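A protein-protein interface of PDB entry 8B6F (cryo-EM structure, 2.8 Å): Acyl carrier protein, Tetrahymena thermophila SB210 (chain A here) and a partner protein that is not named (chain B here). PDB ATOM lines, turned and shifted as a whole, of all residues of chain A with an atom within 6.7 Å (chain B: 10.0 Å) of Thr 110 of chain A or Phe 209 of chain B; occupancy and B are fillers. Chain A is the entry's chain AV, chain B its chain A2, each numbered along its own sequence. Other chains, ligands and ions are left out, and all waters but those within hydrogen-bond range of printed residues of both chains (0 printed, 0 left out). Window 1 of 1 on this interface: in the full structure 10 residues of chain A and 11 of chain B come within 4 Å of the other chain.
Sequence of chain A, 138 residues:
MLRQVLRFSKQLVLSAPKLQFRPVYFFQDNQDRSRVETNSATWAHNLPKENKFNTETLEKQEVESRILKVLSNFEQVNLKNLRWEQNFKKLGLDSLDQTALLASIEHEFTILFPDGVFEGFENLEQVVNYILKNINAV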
ATOM      1  N   ARG A  66      14.816 -25.600  15.213  1.00  0.00           N
ATOM      2  CA  ARG A  66      15.708 -25.131  16.265  1.00  0.00           C
ATOM      3  C   ARG A  66      14.918 -24.432  17.363  1.00  0.00           C
ATOM      4  O   ARG A  66      15.238 -24.571  18.548  1.00  0.00           O
ATOM      5  CB  ARG A  66      16.773 -24.209  15.673  1.00  0.00           C
ATOM      6  CG  ARG A  66      17.691 -24.915  14.681  1.00  0.00           C
ATOM      7  CD  ARG A  66      18.682 -23.963  14.035  1.00  0.00           C
ATOM      8  NE  ARG A  66      19.709 -23.524  14.970  1.00  0.00           N
ATOM      9  CZ  ARG A  66      20.730 -22.742  14.649  1.00  0.00           C
ATOM     10  NH1 ARG A  66      20.898 -22.295  13.416  1.00  0.00           N
ATOM     11  NH2 ARG A  66      21.604 -22.397  15.589  1.00  0.00           N
ATOM     12  N   ILE A 105      16.495 -18.244  22.389  1.00  0.00           N
ATOM     13  CA  ILE A 105      16.512 -18.211  20.930  1.00  0.00           C
ATOM     14  C   ILE A 105      17.665 -17.351  20.432  1.00  0.00           C
ATOM     15  O   ILE A 105      18.327 -17.688  19.444  1.00  0.00           O
ATOM     16  CB  ILE A 105      15.155 -17.722  20.393  1.00  0.00           C
ATOM     17  CG1 ILE A 105      14.065 -18.745  20.721  1.00  0.00           C
ATOM     18  CG2 ILE A 105      15.221 -17.485  18.888  1.00  0.00           C
ATOM     19  CD1 ILE A 105      12.660 -18.264  20.439  1.00  0.00           C
ATOM     20  N   GLU A 106      17.922 -16.223  21.098  1.00  0.00           N
ATOM     21  CA  GLU A 106      19.074 -15.405  20.738  1.00  0.00           C
ATOM     22  C   GLU A 106      20.370 -16.193  20.874  1.00  0.00           C
ATOM     23  O   GLU A 106      21.242 -16.127  20.002  1.00  0.00           O
ATOM     24  CB  GLU A 106      19.127 -14.153  21.613  1.00  0.00           C
ATOM     25  CG  GLU A 106      18.066 -13.118  21.294  1.00  0.00           C
ATOM     26  CD  GLU A 106      18.192 -11.880  22.159  1.00  0.00           C
ATOM     27  OE1 GLU A 106      19.108 -11.836  23.004  1.00  0.00           O
ATOM     28  OE2 GLU A 106      17.379 -10.949  21.996  1.00  0.00           O
ATOM     29  N   HIS A 107      20.512 -16.949  21.964  1.00  0.00           N
ATOM     30  CA  HIS A 107      21.698 -17.780  22.134  1.00  0.00           C
ATOM     31  C   HIS A 107      21.784 -18.836  21.042  1.00  0.00           C
ATOM     32  O   HIS A 107      22.867 -19.101  20.507  1.00  0.00           O
ATOM     33  CB  HIS A 107      21.681 -18.445  23.510  1.00  0.00           C
ATOM     34  CG  HIS A 107      21.816 -17.484  24.649  1.00  0.00           C
ATOM     35  ND1 HIS A 107      22.414 -16.249  24.515  1.00  0.00           N
ATOM     36  CD2 HIS A 107      21.431 -17.578  25.943  1.00  0.00           C
ATOM     37  CE1 HIS A 107      22.389 -15.623  25.678  1.00  0.00           C
ATOM     38  NE2 HIS A 107      21.800 -16.408  26.562  1.00  0.00           N
ATOM     39  N   GLU A 108      20.652 -19.453  20.699  1.00  0.00           N
ATOM     40  CA  GLU A 108      20.663 -20.513  19.699  1.00  0.00           C
ATOM     41  C   GLU A 108      21.117 -19.993  18.342  1.00  0.00           C
ATOM     42  O   GLU A 108      21.919 -20.640  17.659  1.00  0.00           O
ATOM     43  CB  GLU A 108      19.267 -21.131  19.595  1.00  0.00           C
ATOM     44  CG  GLU A 108      19.124 -22.212  18.535  1.00  0.00           C
ATOM     45  CD  GLU A 108      20.011 -23.410  18.797  1.00  0.00           C
ATOM     46  OE1 GLU A 108      20.520 -23.541  19.930  1.00  0.00           O
ATOM     47  OE2 GLU A 108      20.203 -24.221  17.868  1.00  0.00           O
ATOM     48  N   PHE A 109      20.616 -18.832  17.929  1.00  0.00           N
ATOM     49  CA  PHE A 109      20.918 -18.287  16.613  1.00  0.00           C
ATOM     50  C   PHE A 109      22.079 -17.300  16.619  1.00  0.00           C
ATOM     51  O   PHE A 109      22.402 -16.745  15.565  1.00  0.00           O
ATOM     52  CB  PHE A 109      19.669 -17.619  16.033  1.00  0.00           C
ATOM     53  CG  PHE A 109      18.594 -18.593  15.652  1.00  0.00           C
ATOM     54  CD1 PHE A 109      18.589 -19.183  14.402  1.00  0.00           C
ATOM     55  CD2 PHE A 109      17.596 -18.926  16.549  1.00  0.00           C
ATOM     56  CE1 PHE A 109      17.605 -20.083  14.052  1.00  0.00           C
ATOM     57  CE2 PHE A 109      16.609 -19.825  16.206  1.00  0.00           C
ATOM     58  CZ  PHE A 109      16.613 -20.404  14.955  1.00  0.00           C
ATOM     59  N   THR A 110      22.724 -17.082  17.765  1.00  0.00           N
ATOM     60  CA  THR A 110      23.871 -16.179  17.858  1.00  0.00           C
ATOM     61  C   THR A 110      23.523 -14.790  17.328  1.00  0.00           C
ATOM     62  O   THR A 110      24.312 -14.149  16.632  1.00  0.00           O
ATOM     63  CB  THR A 110      25.078 -16.756  17.116  1.00  0.00           C
ATOM     64  OG1 THR A 110      25.210 -18.150  17.425  1.00  0.00           O
ATOM     65  CG2 THR A 110      26.359 -16.037  17.527  1.00  0.00           C
ATOM     66  N   ILE A 111      22.321 -14.319  17.658  1.00  0.00           N
ATOM     67  CA  ILE A 111      21.872 -12.995  17.241  1.00  0.00           C
ATOM     68  C   ILE A 111      21.483 -12.191  18.472  1.00  0.00           C
ATOM     69  O   ILE A 111      21.569 -12.683  19.601  1.00  0.00           O
ATOM     70  CB  ILE A 111      20.697 -13.080  16.249  1.00  0.00           C
ATOM     71  CG1 ILE A 111      19.543 -13.881  16.861  1.00  0.00           C
ATOM     72  CG2 ILE A 111      21.167 -13.688  14.936  1.00  0.00           C
ATOM     73  CD1 ILE A 111      18.319 -13.976  15.981  1.00  0.00           C
ATOM     74  N   LEU A 112      21.055 -10.950  18.260  1.00  0.00           N
ATOM     75  CA  LEU A 112      20.654 -10.069  19.349  1.00  0.00           C
ATOM     76  C   LEU A 112      19.472  -9.236  18.881  1.00  0.00           C
ATOM     77  O   LEU A 112      19.582  -8.502  17.896  1.00  0.00           O
ATOM     78  CB  LEU A 112      21.818  -9.172  19.777  1.00  0.00           C
ATOM     79  CG  LEU A 112      21.775  -8.612  21.196  1.00  0.00           C
ATOM     80  CD1 LEU A 112      21.946  -9.718  22.225  1.00  0.00           C
ATOM     81  CD2 LEU A 112      22.843  -7.555  21.367  1.00  0.00           C
ATOM     82  N   ASN A 136      22.524 -12.446   9.621  1.00  0.00           N
ATOM     83  CA  ASN A 136      23.629 -12.813  10.496  1.00  0.00           C
ATOM     84  C   ASN A 136      23.361 -14.076  11.303  1.00  0.00           C
ATOM     85  O   ASN A 136      24.284 -14.581  11.948  1.00  0.00           O
ATOM     86  CB  ASN A 136      23.939 -11.665  11.458  1.00  0.00           C
ATOM     87  CG  ASN A 136      24.213 -10.362  10.740  1.00  0.00           C
ATOM     88  OD1 ASN A 136      25.298 -10.152  10.205  1.00  0.00           O
ATOM     89  ND2 ASN A 136      23.227  -9.475  10.733  1.00  0.00           N
ATOM     90  N   ALA A 137      22.136 -14.596  11.286  1.00  0.00           N
ATOM     91  CA  ALA A 137      21.826 -15.790  12.060  1.00  0.00           C
ATOM     92  C   ALA A 137      22.712 -16.948  11.622  1.00  0.00           C
ATOM     93  O   ALA A 137      22.881 -17.199  10.425  1.00  0.00           O
ATOM     94  CB  ALA A 137      20.352 -16.157  11.894  1.00  0.00           C
ATOM     95  N   VAL A 138      23.279 -17.652  12.596  1.00  0.00           N
ATOM     96  CA  VAL A 138      24.158 -18.778  12.315  1.00  0.00           C
ATOM     97  C   VAL A 138      23.366 -20.076  12.405  1.00  0.00           C
ATOM     98  O   VAL A 138      23.749 -21.092  11.826  1.00  0.00           O
ATOM     99  CB  VAL A 138      25.363 -18.805  13.278  1.00  0.00           C
ATOM    100  CG1 VAL A 138      26.339 -19.906  12.886  1.00  0.00           C
ATOM    101  CG2 VAL A 138      26.061 -17.457  13.300  1.00  0.00           C
ATOM    102  N   GLN B 199      21.487  -1.659  29.705  1.00  0.00           N
ATOM    103  CA  GLN B 199      22.222  -1.709  28.443  1.00  0.00           C
ATOM    104  C   GLN B 199      21.211  -1.888  27.320  1.00  0.00           C
ATOM    105  O   GLN B 199      20.913  -3.002  26.891  1.00  0.00           O
ATOM    106  CB  GLN B 199      23.253  -2.830  28.451  1.00  0.00           C
ATOM    107  CG  GLN B 199      24.130  -2.842  27.209  1.00  0.00           C
ATOM    108  CD  GLN B 199      25.286  -3.813  27.308  1.00  0.00           C
ATOM    109  OE1 GLN B 199      25.202  -4.826  27.995  1.00  0.00           O
ATOM    110  NE2 GLN B 199      26.377  -3.502  26.622  1.00  0.00           N
ATOM    111  N   ILE B 201      19.715  -2.273  23.819  1.00  0.00           N
ATOM    112  CA  ILE B 201      20.235  -2.859  22.590  1.00  0.00           C
ATOM    113  C   ILE B 201      19.631  -2.082  21.425  1.00  0.00           C
ATOM    114  O   ILE B 201      18.515  -2.360  20.985  1.00  0.00           O
ATOM    115  CB  ILE B 201      19.923  -4.353  22.496  1.00  0.00           C
ATOM    116  CG1 ILE B 201      20.457  -5.095  23.725  1.00  0.00           C
ATOM    117  CG2 ILE B 201      20.517  -4.945  21.228  1.00  0.00           C
ATOM    118  CD1 ILE B 201      21.940  -4.912  23.978  1.00  0.00           C
ATOM    119  N   THR B 202      20.371  -1.095  20.929  1.00  0.00           N
ATOM    120  CA  THR B 202      19.962  -0.352  19.751  1.00  0.00           C
ATOM    121  C   THR B 202      20.377  -1.109  18.491  1.00  0.00           C
ATOM    122  O   THR B 202      21.011  -2.165  18.548  1.00  0.00           O
ATOM    123  CB  THR B 202      20.566   1.051  19.771  1.00  0.00           C
ATOM    124  OG1 THR B 202      21.993   0.958  19.852  1.00  0.00           O
ATOM    125  CG2 THR B 202      20.045   1.839  20.956  1.00  0.00           C
ATOM    126  N   ASN B 203      20.012  -0.562  17.331  1.00  0.00           N
ATOM    127  CA  ASN B 203      20.443  -1.164  16.073  1.00  0.00           C
ATOM    128  C   ASN B 203      21.962  -1.171  15.966  1.00  0.00           C
ATOM    129  O   ASN B 203      22.553  -2.135  15.468  1.00  0.00           O
ATOM    130  CB  ASN B 203      19.828  -0.415  14.892  1.00  0.00           C
ATOM    131  CG  ASN B 203      18.345  -0.673  14.747  1.00  0.00           C
ATOM    132  OD1 ASN B 203      17.654  -0.957  15.724  1.00  0.00           O
ATOM    133  ND2 ASN B 203      17.846  -0.577  13.523  1.00  0.00           N
ATOM    134  N   GLU B 204      22.611  -0.098  16.419  1.00  0.00           N
ATOM    135  CA  GLU B 204      24.068  -0.053  16.386  1.00  0.00           C
ATOM    136  C   GLU B 204      24.673  -1.145  17.257  1.00  0.00           C
ATOM    137  O   GLU B 204      25.630  -1.814  16.852  1.00  0.00           O
ATOM    138  CB  GLU B 204      24.556   1.321  16.841  1.00  0.00           C
ATOM    139  CG  GLU B 204      26.067   1.473  16.830  1.00  0.00           C
ATOM    140  CD  GLU B 204      26.514   2.818  17.354  1.00  0.00           C
ATOM    141  OE1 GLU B 204      25.646   3.691  17.567  1.00  0.00           O
ATOM    142  OE2 GLU B 204      27.732   3.003  17.559  1.00  0.00           O
ATOM    143  N   VAL B 205      24.137  -1.335  18.464  1.00  0.00           N
ATOM    144  CA  VAL B 205      24.669  -2.365  19.353  1.00  0.00           C
ATOM    145  C   VAL B 205      24.445  -3.744  18.754  1.00  0.00           C
ATOM    146  O   VAL B 205      25.333  -4.604  18.788  1.00  0.00           O
ATOM    147  CB  VAL B 205      24.035  -2.246  20.751  1.00  0.00           C
ATOM    148  CG1 VAL B 205      24.514  -3.372  21.657  1.00  0.00           C
ATOM    149  CG2 VAL B 205      24.358  -0.899  21.364  1.00  0.00           C
ATOM    150  N   ALA B 206      23.255  -3.982  18.202  1.00  0.00           N
ATOM    151  CA  ALA B 206      22.976  -5.275  17.589  1.00  0.00           C
ATOM    152  C   ALA B 206      23.905  -5.534  16.413  1.00  0.00           C
ATOM    153  O   ALA B 206      24.404  -6.651  16.240  1.00  0.00           O
ATOM    154  CB  ALA B 206      21.516  -5.339  17.143  1.00  0.00           C
ATOM    155  N   GLN B 207      24.155  -4.511  15.596  1.00  0.00           N
ATOM    156  CA  GLN B 207      25.036  -4.685  14.447  1.00  0.00           C
ATOM    157  C   GLN B 207      26.478  -4.903  14.886  1.00  0.00           C
ATOM    158  O   GLN B 207      27.210  -5.677  14.261  1.00  0.00           O
ATOM    159  CB  GLN B 207      24.930  -3.480  13.516  1.00  0.00           C
ATOM    160  CG  GLN B 207      25.805  -3.583  12.276  1.00  0.00           C
ATOM    161  CD  GLN B 207      25.620  -4.894  11.538  1.00  0.00           C
ATOM    162  OE1 GLN B 207      26.586  -5.507  11.088  1.00  0.00           O
ATOM    163  NE2 GLN B 207      24.373  -5.330  11.407  1.00  0.00           N
ATOM    164  N   ASN B 208      26.909  -4.228  15.954  1.00  0.00           N
ATOM    165  CA  ASN B 208      28.245  -4.479  16.482  1.00  0.00           C
ATOM    166  C   ASN B 208      28.374  -5.917  16.964  1.00  0.00           C
ATOM    167  O   ASN B 208      29.395  -6.571  16.723  1.00  0.00           O
ATOM    168  CB  ASN B 208      28.560  -3.507  17.618  1.00  0.00           C
ATOM    169  CG  ASN B 208      28.604  -2.066  17.158  1.00  0.00           C
ATOM    170  OD1 ASN B 208      28.814  -1.784  15.979  1.00  0.00           O
ATOM    171  ND2 ASN B 208      28.419  -1.143  18.092  1.00  0.00           N
ATOM    172  N   PHE B 209      27.354  -6.421  17.660  1.00  0.00           N
ATOM    173  CA  PHE B 209      27.373  -7.813  18.092  1.00  0.00           C
ATOM    174  C   PHE B 209      27.448  -8.751  16.895  1.00  0.00           C
ATOM    175  O   PHE B 209      28.231  -9.708  16.892  1.00  0.00           O
ATOM    176  CB  PHE B 209      26.132  -8.110  18.933  1.00  0.00           C
ATOM    177  CG  PHE B 209      26.105  -9.495  19.514  1.00  0.00           C
ATOM    178  CD1 PHE B 209      25.607 -10.560  18.783  1.00  0.00           C
ATOM    179  CD2 PHE B 209      26.560  -9.727  20.800  1.00  0.00           C
ATOM    180  CE1 PHE B 209      25.576 -11.832  19.317  1.00  0.00           C
ATOM    181  CE2 PHE B 209      26.531 -10.999  21.340  1.00  0.00           C
ATOM    182  CZ  PHE B 209      26.039 -12.052  20.596  1.00  0.00           C
ATOM    183  N   ALA B 210      26.647  -8.484  15.862  1.00  0.00           N
ATOM    184  CA  ALA B 210      26.656  -9.335  14.677  1.00  0.00           C
ATOM    185  C   ALA B 210      28.011  -9.310  13.985  1.00  0.00           C
ATOM    186  O   ALA B 210      28.520 -10.354  13.564  1.00  0.00           O
ATOM    187  CB  ALA B 210      25.556  -8.899  13.712  1.00  0.00           C
ATOM    188  N   ASN B 211      28.614  -8.127  13.859  1.00  0.00           N
ATOM    189  CA  ASN B 211      29.930  -8.039  13.234  1.00  0.00           C
ATOM    190  C   ASN B 211      30.970  -8.808  14.038  1.00  0.00           C
ATOM    191  O   ASN B 211      31.825  -9.492  13.463  1.00  0.00           O
ATOM    192  CB  ASN B 211      30.351  -6.578  13.080  1.00  0.00           C
ATOM    193  CG  ASN B 211      29.377  -5.775  12.238  1.00  0.00           C
ATOM    194  OD1 ASN B 211      29.035  -4.644  12.579  1.00  0.00           O
ATOM    195  ND2 ASN B 211      28.923  -6.359  11.134  1.00  0.00           N
ATOM    196  N   HIS B 212      30.917  -8.708  15.365  1.00  0.00           N
ATOM    197  CA  HIS B 212      31.859  -9.450  16.194  1.00  0.00           C
ATOM    198  C   HIS B 212      31.688 -10.952  16.014  1.00  0.00           C
ATOM    199  O   HIS B 212      32.676 -11.690  15.919  1.00  0.00           O
ATOM    200  CB  HIS B 212      31.680  -9.068  17.663  1.00  0.00           C
ATOM    201  CG  HIS B 212      32.641  -9.756  18.582  1.00  0.00           C
ATOM    202  ND1 HIS B 212      33.977  -9.421  18.648  1.00  0.00           N
ATOM    203  CD2 HIS B 212      32.463 -10.765  19.467  1.00  0.00           C
ATOM    204  CE1 HIS B 212      34.578 -10.191  19.535  1.00  0.00           C
ATOM    205  NE2 HIS B 212      33.683 -11.015  20.046  1.00  0.00           N
ATOM    206  N   GLN B 213      30.443 -11.427  15.967  1.00  0.00           N
ATOM    207  CA  GLN B 213      30.208 -12.860  15.822  1.00  0.00           C
ATOM    208  C   GLN B 213      30.597 -13.361  14.437  1.00  0.00           C
ATOM    209  O   GLN B 213      31.010 -14.516  14.293  1.00  0.00           O
ATOM    210  CB  GLN B 213      28.743 -13.181  16.108  1.00  0.00           C
ATOM    211  CG  GLN B 213      28.309 -12.859  17.528  1.00  0.00           C
ATOM    212  CD  GLN B 213      29.082 -13.641  18.569  1.00  0.00           C
ATOM    213  OE1 GLN B 213      29.288 -14.845  18.431  1.00  0.00           O
ATOM    214  NE2 GLN B 213      29.523 -12.955  19.616  1.00  0.00           N
ATOM    215  N   ASN B 214      30.471 -12.518  13.409  1.00  0.00           N
ATOM    216  CA  ASN B 214      30.811 -12.950  12.057  1.00  0.00           C
ATOM    217  C   ASN B 214      32.276 -13.351  11.945  1.00  0.00           C
ATOM    218  O   ASN B 214      32.633 -14.151  11.073  1.00  0.00           O
ATOM    219  CB  ASN B 214      30.486 -11.846  11.053  1.00  0.00           C
ATOM    220  CG  ASN B 214      28.996 -11.614  10.904  1.00  0.00           C
ATOM    221  OD1 ASN B 214      28.192 -12.177  11.646  1.00  0.00           O
ATOM    222  ND2 ASN B 214      28.620 -10.783   9.940  1.00  0.00           N
ATOM    223  N   ASN B 215      33.138 -12.805  12.805  1.00  0.00           N
ATOM    224  CA  ASN B 215      34.538 -13.220  12.809  1.00  0.00           C
ATOM    225  C   ASN B 215      34.676 -14.684  13.209  1.00  0.00           C
ATOM    226  O   ASN B 215      35.484 -15.421  12.632  1.00  0.00           O
ATOM    227  CB  ASN B 215      35.351 -12.335  13.752  1.00  0.00           C
ATOM    228  CG  ASN B 215      35.479 -10.914  13.251  1.00  0.00           C
ATOM    229  OD1 ASN B 215      34.651 -10.058  13.557  1.00  0.00           O
ATOM    230  ND2 ASN B 215      36.526 -10.652  12.477  1.00  0.00           N
ATOM    231  N   ASP B 216      33.897 -15.121  14.193  1.00  0.00           N
ATOM    232  CA  ASP B 216      33.923 -16.494  14.675  1.00  0.00           C
ATOM    233  C   ASP B 216      32.868 -17.368  14.011  1.00  0.00           C
ATOM    234  O   ASP B 216      32.649 -18.497  14.459  1.00  0.00           O
ATOM    235  CB  ASP B 216      33.728 -16.517  16.192  1.00  0.00           C
ATOM    236  CG  ASP B 216      34.809 -15.757  16.930  1.00  0.00           C
ATOM    237  OD1 ASP B 216      35.996 -15.918  16.580  1.00  0.00           O
ATOM    238  OD2 ASP B 216      34.470 -14.987  17.854  1.00  0.00           O
ATOM    239  N   ARG B 217      32.214 -16.871  12.960  1.00  0.00           N
ATOM    240  CA  ARG B 217      31.172 -17.643  12.289  1.00  0.00           C
ATOM    241  C   ARG B 217      31.646 -19.045  11.929  1.00  0.00           C
ATOM    242  O   ARG B 217      30.891 -20.015  12.060  1.00  0.00           O
ATOM    243  CB  ARG B 217      30.708 -16.902  11.035  1.00  0.00           C
ATOM    244  CG  ARG B 217      29.895 -17.754  10.072  1.00  0.00           C
ATOM    245  CD  ARG B 217      29.319 -16.911   8.950  1.00  0.00           C
ATOM    246  NE  ARG B 217      28.335 -15.952   9.438  1.00  0.00           N
ATOM    247  CZ  ARG B 217      27.051 -16.222   9.630  1.00  0.00           C
ATOM    248  NH1 ARG B 217      26.553 -17.424   9.391  1.00  0.00           N
ATOM    249  NH2 ARG B 217      26.246 -15.261  10.072  1.00  0.00           N
ATOM    250  N   TRP B 218      32.889 -19.175  11.466  1.00  0.00           N
ATOM    251  CA  TRP B 218      33.371 -20.482  11.032  1.00  0.00           C
ATOM    252  C   TRP B 218      33.352 -21.487  12.176  1.00  0.00           C
ATOM    253  O   TRP B 218      32.960 -22.644  11.990  1.00  0.00           O
ATOM    254  CB  TRP B 218      34.779 -20.359  10.453  1.00  0.00           C
ATOM    255  CG  TRP B 218      35.342 -21.666   9.989  1.00  0.00           C
ATOM    256  CD1 TRP B 218      34.983 -22.358   8.872  1.00  0.00           C
ATOM    257  CD2 TRP B 218      36.366 -22.439  10.628  1.00  0.00           C
ATOM    258  NE1 TRP B 218      35.718 -23.513   8.774  1.00  0.00           N
ATOM    259  CE2 TRP B 218      36.575 -23.586   9.839  1.00  0.00           C
ATOM    260  CE3 TRP B 218      37.128 -22.270  11.788  1.00  0.00           C
ATOM    261  CZ2 TRP B 218      37.510 -24.561  10.173  1.00  0.00           C
ATOM    262  CZ3 TRP B 218      38.056 -23.240  12.119  1.00  0.00           C
ATOM    263  CH2 TRP B 218      38.240 -24.372  11.314  1.00  0.00           C
ATOM    264  N   VAL B 219      33.778 -21.066  13.368  1.00  0.00           N
ATOM    265  CA  VAL B 219      33.831 -21.986  14.499  1.00  0.00           C
ATOM    266  C   VAL B 219      32.429 -22.411  14.913  1.00  0.00           C
ATOM    267  O   VAL B 219      32.207 -23.562  15.304  1.00  0.00           O
ATOM    268  CB  VAL B 219      34.595 -21.341  15.671  1.00  0.00           C
ATOM    269  CG1 VAL B 219      34.679 -22.298  16.850  1.00  0.00           C
ATOM    270  CG2 VAL B 219      35.986 -20.917  15.228  1.00  0.00           C
ATOM    271  N   TYR B 220      31.463 -21.492  14.844  1.00  0.00           N
ATOM    272  CA  TYR B 220      30.104 -21.825  15.261  1.00  0.00           C
ATOM    273  C   TYR B 220      29.509 -22.924  14.391  1.00  0.00           C
ATOM    274  O   TYR B 220      28.853 -23.840  14.898  1.00  0.00           O
ATOM    275  CB  TYR B 220      29.222 -20.577  15.216  1.00  0.00           C
ATOM    276  CG  TYR B 220      29.548 -19.561  16.282  1.00  0.00           C
ATOM    277  CD1 TYR B 220      29.277 -19.818  17.620  1.00  0.00           C
ATOM    278  CD2 TYR B 220      30.109 -18.338  15.950  1.00  0.00           C
ATOM    279  CE1 TYR B 220      29.569 -18.886  18.600  1.00  0.00           C
ATOM    280  CE2 TYR B 220      30.404 -17.401  16.921  1.00  0.00           C
ATOM    281  CZ  TYR B 220      30.132 -17.680  18.243  1.00  0.00           C
ATOM    282  OH  TYR B 220      30.421 -16.747  19.211  1.00  0.00           O
ATOM    283  N   GLU B 221      29.720 -22.849  13.081  1.00  0.00           N
ATOM    284  CA  GLU B 221      29.142 -23.806  12.149  1.00  0.00           C
ATOM    285  C   GLU B 221      30.045 -25.003  11.888  1.00  0.00           C
ATOM    286  O   GLU B 221      29.672 -25.880  11.102  1.00  0.00           O
ATOM    287  CB  GLU B 221      28.813 -23.113  10.823  1.00  0.00           C
ATOM    288  CG  GLU B 221      30.027 -22.586  10.079  1.00  0.00           C
ATOM    289  CD  GLU B 221      29.649 -21.833   8.821  1.00  0.00           C
ATOM    290  OE1 GLU B 221      28.453 -21.512   8.659  1.00  0.00           O
ATOM    291  OE2 GLU B 221      30.545 -21.567   7.993  1.00  0.00           O
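Among the printed residues, pairs that only touch across the chains: Thr 110 of chain A with Gln 213 of chain B (3.3 Å), Leu 112 of chain A with Ile 201 of chain B (3.5 Å), Asn 136 of chain A with Ala 210 of chain B (3.6 Å), Thr 110 of chain A with Phe 209 of chain B (3.8 Å), Val 138 of chain A with Tyr 220 of chain B (3.8 Å), Leu 112 of chain A with Ala 206 of chain B (3.8 Å), Ala 137 of chain A with Arg 217 of chain B (3.8 Å) and Val 138 of chain A with Arg 217 of chain B (3.9 Å).
O of Ala 210 of chain B lies close to OD1 of Asn 214 of chain B (2.7 Å).
O of Phe 109 of chain A is in hydrogen-bond range of N of Val 138 of chain A (3.2 Å).
The guanidinium group (NH1) of Arg 66 of chain A sits close to the backbone carbonyl oxygen (O) of Val 138 of chain A (3.5 Å).
ND2 of Asn 214 of chain B sits at hydrogen-bond distance from OD1 of Asn 136 of chain A (3.4 Å).
The guanidinium group of Arg 217 of chain B is in hydrogen-bond range of the backbone carbonyl oxygen of Asn 136 of chain A (2.8 Å).
Of the 12 printed residues of chain A, 5 touch a printed residue of chain B.
Printed residues of chain B that touch a printed residue of chain A: Ile 201, Ala 206, Phe 209, Ala 210, Gln 213, Asn 214, Arg 217 and Tyr 220.
Hydrophobic or aromatic side chains of chain B within 4 Å of the printed part of chain A: Ile 201, Ala 206, Phe 209, Ala 210 and Tyr 220.
Among the printed residues, 10 pairs touch across the chains.
Ile 105 of chain A touches none of the printed residues of chain B.
Thr 110 of chain A touches two residues of chain B.
Of the printed residues of chain B, Ala 137 of chain A touches Arg 217 (3.8 Å).
Of the printed residues of chain A, Ala 206 of chain B touches Leu 112 (3.8 Å).
Gln 207 of chain B touches none of the printed residues of chain A.
Phe 209 of chain B touches just one residue of chain A: Thr 110 (3.8 Å).
Of the printed residues of chain A, Gln 213 of chain B touches Thr 110 (3.3 Å).
Printed residues of chain A within 4 Å of Asn 214 of chain B: Asn 136 (3.4 Å).
Of the printed residues of chain A, Tyr 220 of chain B touches Val 138.
The nearest printed residue of chain A that does not touch Phe 209 of chain B is Ile 111 of chain A (4.1 Å).
The nearest printed residue of chain A that does not touch Gln 213 of chain B is Val 138 of chain A (5.8 Å).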
